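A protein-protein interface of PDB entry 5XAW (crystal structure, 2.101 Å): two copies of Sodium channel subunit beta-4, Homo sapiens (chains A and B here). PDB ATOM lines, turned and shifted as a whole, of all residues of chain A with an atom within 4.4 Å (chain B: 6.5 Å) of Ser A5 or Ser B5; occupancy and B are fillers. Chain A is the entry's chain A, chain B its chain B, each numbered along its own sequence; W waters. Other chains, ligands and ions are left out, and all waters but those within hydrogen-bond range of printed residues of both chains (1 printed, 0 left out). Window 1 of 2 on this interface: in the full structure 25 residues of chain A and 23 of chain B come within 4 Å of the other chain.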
ATOM      1  N   VAL A   4      -6.591 -12.017   6.421  1.00  0.00           N
ATOM      2  CA  VAL A   4      -5.804 -11.308   5.418  1.00  0.00           C
ATOM      3  C   VAL A   4      -6.158  -9.822   5.444  1.00  0.00           C
ATOM      4  O   VAL A   4      -7.211  -9.407   5.936  1.00  0.00           O
ATOM      5  CB  VAL A   4      -6.017 -11.889   4.009  1.00  0.00           C
ATOM      6  CG1 VAL A   4      -5.692 -13.375   3.998  1.00  0.00           C
ATOM      7  CG2 VAL A   4      -7.440 -11.632   3.552  1.00  0.00           C
ATOM      8  N   SER A   5      -5.268  -9.016   4.874  1.00  0.00           N
ATOM      9  CA  SER A   5      -5.453  -7.573   4.865  1.00  0.00           C
ATOM     10  C   SER A   5      -4.778  -6.998   3.628  1.00  0.00           C
ATOM     11  O   SER A   5      -3.801  -7.560   3.120  1.00  0.00           O
ATOM     12  CB  SER A   5      -4.889  -6.951   6.151  1.00  0.00           C
ATOM     13  OG  SER A   5      -4.555  -5.577   6.010  1.00  0.00           O
ATOM     14  N   VAL A   6      -5.308  -5.873   3.142  1.00  0.00           N
ATOM     15  CA  VAL A   6      -4.622  -5.131   2.093  1.00  0.00           C
ATOM     16  C   VAL A   6      -3.715  -4.070   2.717  1.00  0.00           C
ATOM     17  O   VAL A   6      -3.162  -3.225   2.007  1.00  0.00           O
ATOM     18  CB  VAL A   6      -5.615  -4.509   1.089  1.00  0.00           C
ATOM     19  CG1 VAL A   6      -6.452  -5.602   0.379  1.00  0.00           C
ATOM     20  CG2 VAL A   6      -6.513  -3.472   1.760  1.00  0.00           C
ATOM     21  N   GLY A   7      -3.534  -4.103   4.034  1.00  0.00           N
ATOM     22  CA  GLY A   7      -2.543  -3.253   4.674  1.00  0.00           C
ATOM     23  C   GLY A   7      -3.153  -2.213   5.596  1.00  0.00           C
ATOM     24  O   GLY A   7      -4.269  -2.363   6.096  1.00  0.00           O
ATOM     25  N   PRO A  23     -12.296   3.073   6.184  1.00  0.00           N
ATOM     26  CA  PRO A  23     -12.199   1.778   6.871  1.00  0.00           C
ATOM     27  C   PRO A  23     -11.056   1.699   7.868  1.00  0.00           C
ATOM     28  O   PRO A  23      -9.928   2.131   7.604  1.00  0.00           O
ATOM     29  CB  PRO A  23     -11.959   0.789   5.718  1.00  0.00           C
ATOM     30  CG  PRO A  23     -11.187   1.622   4.700  1.00  0.00           C
ATOM     31  CD  PRO A  23     -11.810   3.007   4.793  1.00  0.00           C
ATOM     32  N   CYS A  24     -11.354   1.093   9.014  1.00  0.00           N
ATOM     33  CA  CYS A  24     -10.301   0.655   9.921  1.00  0.00           C
ATOM     34  C   CYS A  24     -10.843  -0.452  10.805  1.00  0.00           C
ATOM     35  O   CYS A  24     -11.830  -0.246  11.523  1.00  0.00           O
ATOM     36  CB  CYS A  24      -9.773   1.803  10.778  1.00  0.00           C
ATOM     37  SG  CYS A  24      -8.568   1.210  11.977  1.00  0.00           S
ATOM     38  N   THR A  25     -10.192  -1.607  10.764  1.00  0.00           N
ATOM     39  CA  THR A  25     -10.488  -2.732  11.632  1.00  0.00           C
ATOM     40  C   THR A  25      -9.239  -3.088  12.416  1.00  0.00           C
ATOM     41  O   THR A  25      -8.126  -2.669  12.087  1.00  0.00           O
ATOM     42  CB  THR A  25     -10.963  -3.956  10.836  1.00  0.00           C
ATOM     43  OG1 THR A  25      -9.915  -4.381   9.954  1.00  0.00           O
ATOM     44  CG2 THR A  25     -12.183  -3.618  10.029  1.00  0.00           C
ATOM     45  N   GLU B   3      -3.035  -5.381  15.854  1.00  0.00           N
ATOM     46  CA  GLU B   3      -2.675  -4.720  14.607  1.00  0.00           C
ATOM     47  C   GLU B   3      -3.924  -4.231  13.882  1.00  0.00           C
ATOM     48  O   GLU B   3      -5.017  -4.791  14.027  1.00  0.00           O
ATOM     49  CB  GLU B   3      -1.881  -5.649  13.690  1.00  0.00           C
ATOM     50  CG  GLU B   3      -2.757  -6.587  12.894  1.00  0.00           C
ATOM     51  CD  GLU B   3      -2.564  -8.038  13.284  1.00  0.00           C
ATOM     52  OE1 GLU B   3      -2.686  -8.391  14.484  1.00  0.00           O
ATOM     53  OE2 GLU B   3      -2.266  -8.836  12.377  1.00  0.00           O
ATOM     54  N   VAL B   4      -3.733  -3.189  13.076  1.00  0.00           N
ATOM     55  CA  VAL B   4      -4.821  -2.487  12.411  1.00  0.00           C
ATOM     56  C   VAL B   4      -4.802  -2.773  10.909  1.00  0.00           C
ATOM     57  O   VAL B   4      -3.785  -3.165  10.332  1.00  0.00           O
ATOM     58  CB  VAL B   4      -4.733  -0.976  12.684  1.00  0.00           C
ATOM     59  CG1 VAL B   4      -4.529  -0.739  14.175  1.00  0.00           C
ATOM     60  CG2 VAL B   4      -3.589  -0.374  11.895  1.00  0.00           C
ATOM     61  N   SER B   5      -5.947  -2.545  10.268  1.00  0.00           N
ATOM     62  CA  SER B   5      -6.092  -2.838   8.849  1.00  0.00           C
ATOM     63  C   SER B   5      -7.113  -1.890   8.232  1.00  0.00           C
ATOM     64  O   SER B   5      -8.050  -1.446   8.902  1.00  0.00           O
ATOM     65  CB  SER B   5      -6.515  -4.298   8.648  1.00  0.00           C
ATOM     66  OG  SER B   5      -7.139  -4.513   7.397  1.00  0.00           O
ATOM     67  N   VAL B   6      -6.932  -1.590   6.944  1.00  0.00           N
ATOM     68  CA  VAL B   6      -7.955  -0.841   6.228  1.00  0.00           C
ATOM     69  C   VAL B   6      -8.888  -1.826   5.527  1.00  0.00           C
ATOM     70  O   VAL B   6      -9.726  -1.424   4.719  1.00  0.00           O
ATOM     71  CB  VAL B   6      -7.344   0.184   5.250  1.00  0.00           C
ATOM     72  CG1 VAL B   6      -6.504   1.209   6.014  1.00  0.00           C
ATOM     73  CG2 VAL B   6      -6.504  -0.486   4.150  1.00  0.00           C
ATOM     74  N   GLY B   7      -8.781  -3.112   5.846  1.00  0.00           N
ATOM     75  CA  GLY B   7      -9.748  -4.085   5.364  1.00  0.00           C
ATOM     76  C   GLY B   7      -9.159  -5.074   4.373  1.00  0.00           C
ATOM     77  O   GLY B   7      -7.954  -5.324   4.347  1.00  0.00           O
ATOM     78  N   LYS B   8     -10.045  -5.666   3.563  1.00  0.00           N
ATOM     79  CA  LYS B   8      -9.675  -6.741   2.644  1.00  0.00           C
ATOM     80  C   LYS B   8      -9.895  -6.382   1.180  1.00  0.00           C
ATOM     81  O   LYS B   8      -9.764  -7.255   0.309  1.00  0.00           O
ATOM     82  CB  LYS B   8     -10.452  -8.023   2.968  1.00  0.00           C
ATOM     83  CG  LYS B   8     -10.266  -8.528   4.384  1.00  0.00           C
ATOM     84  CD  LYS B   8     -11.153  -9.760   4.608  1.00  0.00           C
ATOM     85  CE  LYS B   8     -11.460  -9.940   6.081  1.00  0.00           C
ATOM     86  NZ  LYS B   8     -10.242 -10.384   6.813  1.00  0.00           N
ATOM     87  N   ALA B   9     -10.227  -5.131   0.881  1.00  0.00           N
ATOM     88  CA  ALA B   9     -10.486  -4.734  -0.490  1.00  0.00           C
ATOM     89  C   ALA B   9     -10.015  -3.302  -0.676  1.00  0.00           C
ATOM     90  O   ALA B   9     -10.073  -2.488   0.249  1.00  0.00           O
ATOM     91  CB  ALA B   9     -11.972  -4.870  -0.857  1.00  0.00           C
ATOM     92  N   PRO B  23      -1.142  -5.062  -2.629  1.00  0.00           N
ATOM     93  CA  PRO B  23      -0.870  -5.496  -1.254  1.00  0.00           C
ATOM     94  C   PRO B  23      -1.708  -6.685  -0.808  1.00  0.00           C
ATOM     95  O   PRO B  23      -2.919  -6.765  -1.050  1.00  0.00           O
ATOM     96  CB  PRO B  23      -1.212  -4.251  -0.422  1.00  0.00           C
ATOM     97  CG  PRO B  23      -2.266  -3.546  -1.249  1.00  0.00           C
ATOM     98  CD  PRO B  23      -1.877  -3.788  -2.685  1.00  0.00           C
ATOM     99  N   CYS B  24      -1.044  -7.603  -0.116  1.00  0.00           N
ATOM    100  CA  CYS B  24      -1.761  -8.585   0.688  1.00  0.00           C
ATOM    101  C   CYS B  24      -0.836  -9.092   1.775  1.00  0.00           C
ATOM    102  O   CYS B  24       0.246  -9.612   1.483  1.00  0.00           O
ATOM    103  CB  CYS B  24      -2.271  -9.743  -0.156  1.00  0.00           C
ATOM    104  SG  CYS B  24      -3.129 -10.920   0.886  1.00  0.00           S
ATOM    105  N   THR B  25      -1.262  -8.930   3.020  1.00  0.00           N
ATOM    106  CA  THR B  25      -0.583  -9.476   4.179  1.00  0.00           C
ATOM    107  C   THR B  25      -1.590 -10.307   4.950  1.00  0.00           C
ATOM    108  O   THR B  25      -2.801 -10.140   4.804  1.00  0.00           O
ATOM    109  CB  THR B  25       0.003  -8.373   5.089  1.00  0.00           C
ATOM    110  OG1 THR B  25      -1.059  -7.624   5.698  1.00  0.00           O
ATOM    111  CG2 THR B  25       0.859  -7.435   4.288  1.00  0.00           C
ATOM    112  N   PHE B  26      -1.084 -11.225   5.759  1.00  0.00           N
ATOM    113  CA  PHE B  26      -1.969 -12.045   6.562  1.00  0.00           C
ATOM    114  C   PHE B  26      -1.365 -12.205   7.945  1.00  0.00           C
ATOM    115  O   PHE B  26      -0.145 -12.133   8.124  1.00  0.00           O
ATOM    116  CB  PHE B  26      -2.220 -13.419   5.925  1.00  0.00           C
ATOM    117  CG  PHE B  26      -0.981 -14.247   5.786  1.00  0.00           C
ATOM    118  CD1 PHE B  26      -0.142 -14.085   4.694  1.00  0.00           C
ATOM    119  CD2 PHE B  26      -0.636 -15.168   6.765  1.00  0.00           C
ATOM    120  CE1 PHE B  26       1.008 -14.832   4.571  1.00  0.00           C
ATOM    121  CE2 PHE B  26       0.513 -15.921   6.652  1.00  0.00           C
ATOM    122  CZ  PHE B  26       1.336 -15.760   5.554  1.00  0.00           C
ATOM    123  N   SER B  27      -2.240 -12.414   8.922  1.00  0.00           N
ATOM    124  CA  SER B  27      -1.841 -12.575  10.307  1.00  0.00           C
ATOM    125  C   SER B  27      -2.328 -13.919  10.827  1.00  0.00           C
ATOM    126  O   SER B  27      -3.375 -14.431  10.411  1.00  0.00           O
ATOM    127  CB  SER B  27      -2.395 -11.456  11.182  1.00  0.00           C
ATOM    128  OG  SER B  27      -3.808 -11.393  11.089  1.00  0.00           O
ATOM    129  N   ALA B 116      -8.141 -11.464  -0.341  1.00  0.00           N
ATOM    130  CA  ALA B 116      -8.144 -10.014  -0.467  1.00  0.00           C
ATOM    131  C   ALA B 116      -8.312  -9.645  -1.936  1.00  0.00           C
ATOM    132  O   ALA B 116      -7.836 -10.355  -2.829  1.00  0.00           O
ATOM    133  CB  ALA B 116      -6.855  -9.405   0.095  1.00  0.00           C
HETATM  134  O   HOH W   1      -9.780 -13.106   6.044  1.00  0.00           O
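Water W1 bridges NZ of Lys B8 and N of Val A4.
Of the 7 printed residues of chain A, 7 touch a printed residue of chain B.
Hydrophobic or aromatic side chains of chain A within 4 Å of the printed part of chain B: Val A4, Val A6 and Pro A23.
Along chain A the printed residues that touch a printed residue of chain B span positions 4 to 25.
Hydrophobic or aromatic side chains of chain B within 4 Å of the printed part of chain A: Val B4, Val B6, Pro B23, Phe B26 and Ala B116.
O of Val A4 is in hydrogen-bond range of NZ of Lys B8.
The backbone NH of Val A6 is in hydrogen-bond range of the backbone carbonyl oxygen of Gly B7 (3.0 Å).
The backbone carbonyl oxygen (O) of Thr A25 is in hydrogen-bond range of the backbone NH (N) of Ser B5 (2.8 Å).
The backbone carbonyl oxygen (O) of Gly A7 sits at hydrogen-bond distance from the backbone NH (N) of Val B6 (2.9 Å).
The backbone NH of Ser A5 is in hydrogen-bond range of the backbone carbonyl oxygen of Thr B25 (2.7 Å).
OG of Ser A5 is in hydrogen-bond range of OG of Ser B5.
O of Gly B7 touches CA of Ser A5 (3.4 Å).
O of Ser A5 touches CA of Cys B24, at 3.3 Å.
Val B6 touches Val A6 (CG2 to CG2, 3.8 Å).
Val A6 touches Lys B8 (CG1 to C, 3.6 Å).
Ala B9 touches Val A6 (N to CG1, 3.8 Å).
Val A6 touches Ala B116 (CG1 to CB, 3.8 Å).
Ser B5 touches Gly A7 (CA to O, 3.3 Å).
Pro A23 touches Val B6 (CB to O, 3.3 Å).
Ser B5 touches Cys A24 (O to CA, 3.2 Å).
Val B4 touches Thr A25 (CA to O, 3.3 Å).
Of chain B, only Ser B5 (3.1 Å), Gly B7 (3.4 Å), Cys B24 (3.3 Å) and Thr B25 (2.7 Å) come within 4 Å of Ser A5.
Printed residues of chain A within 4 Å of Cys B24: Ser A5 (3.3 Å).
Printed residues of chain B within 4 Å of Val A6: Val B6, Gly B7, Lys B8, Ala B9, Pro B23 and Ala B116.
Of the printed residues of chain A, Ala B116 touches Val A4 (3.96 Å) and Val A6 (3.8 Å).
Printed residues of chain A within 4 Å of Lys B8: Val A4 and Val A6.
Of the printed residues of chain A, Val B4 touches Thr A25.
The nearest residue of chain A that does not touch Ser B5 is Pro A23 (4.2 Å).
The nearest printed residue of chain B that does not touch Cys A24 is Val B4 (4.5 Å).
The side-chain hydroxyl of Ser B5 is in hydrogen-bond range of the backbone NH of Gly B7, at 2.7 Å.
The side-chain hydroxyl (OG) of Ser A5 is in hydrogen-bond range of the backbone NH (N) of Gly A7 (2.7 Å).
Ser A5 touches its own counterpart, Ser B5.
Val A6 touches its own counterpart, Val B6.
Val A6 touches Gly B7, and with the chains exchanged Gly A7 touches Val B6.
Val A6 touches Pro B23, and with the chains exchanged Pro A23 touches Val B6.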
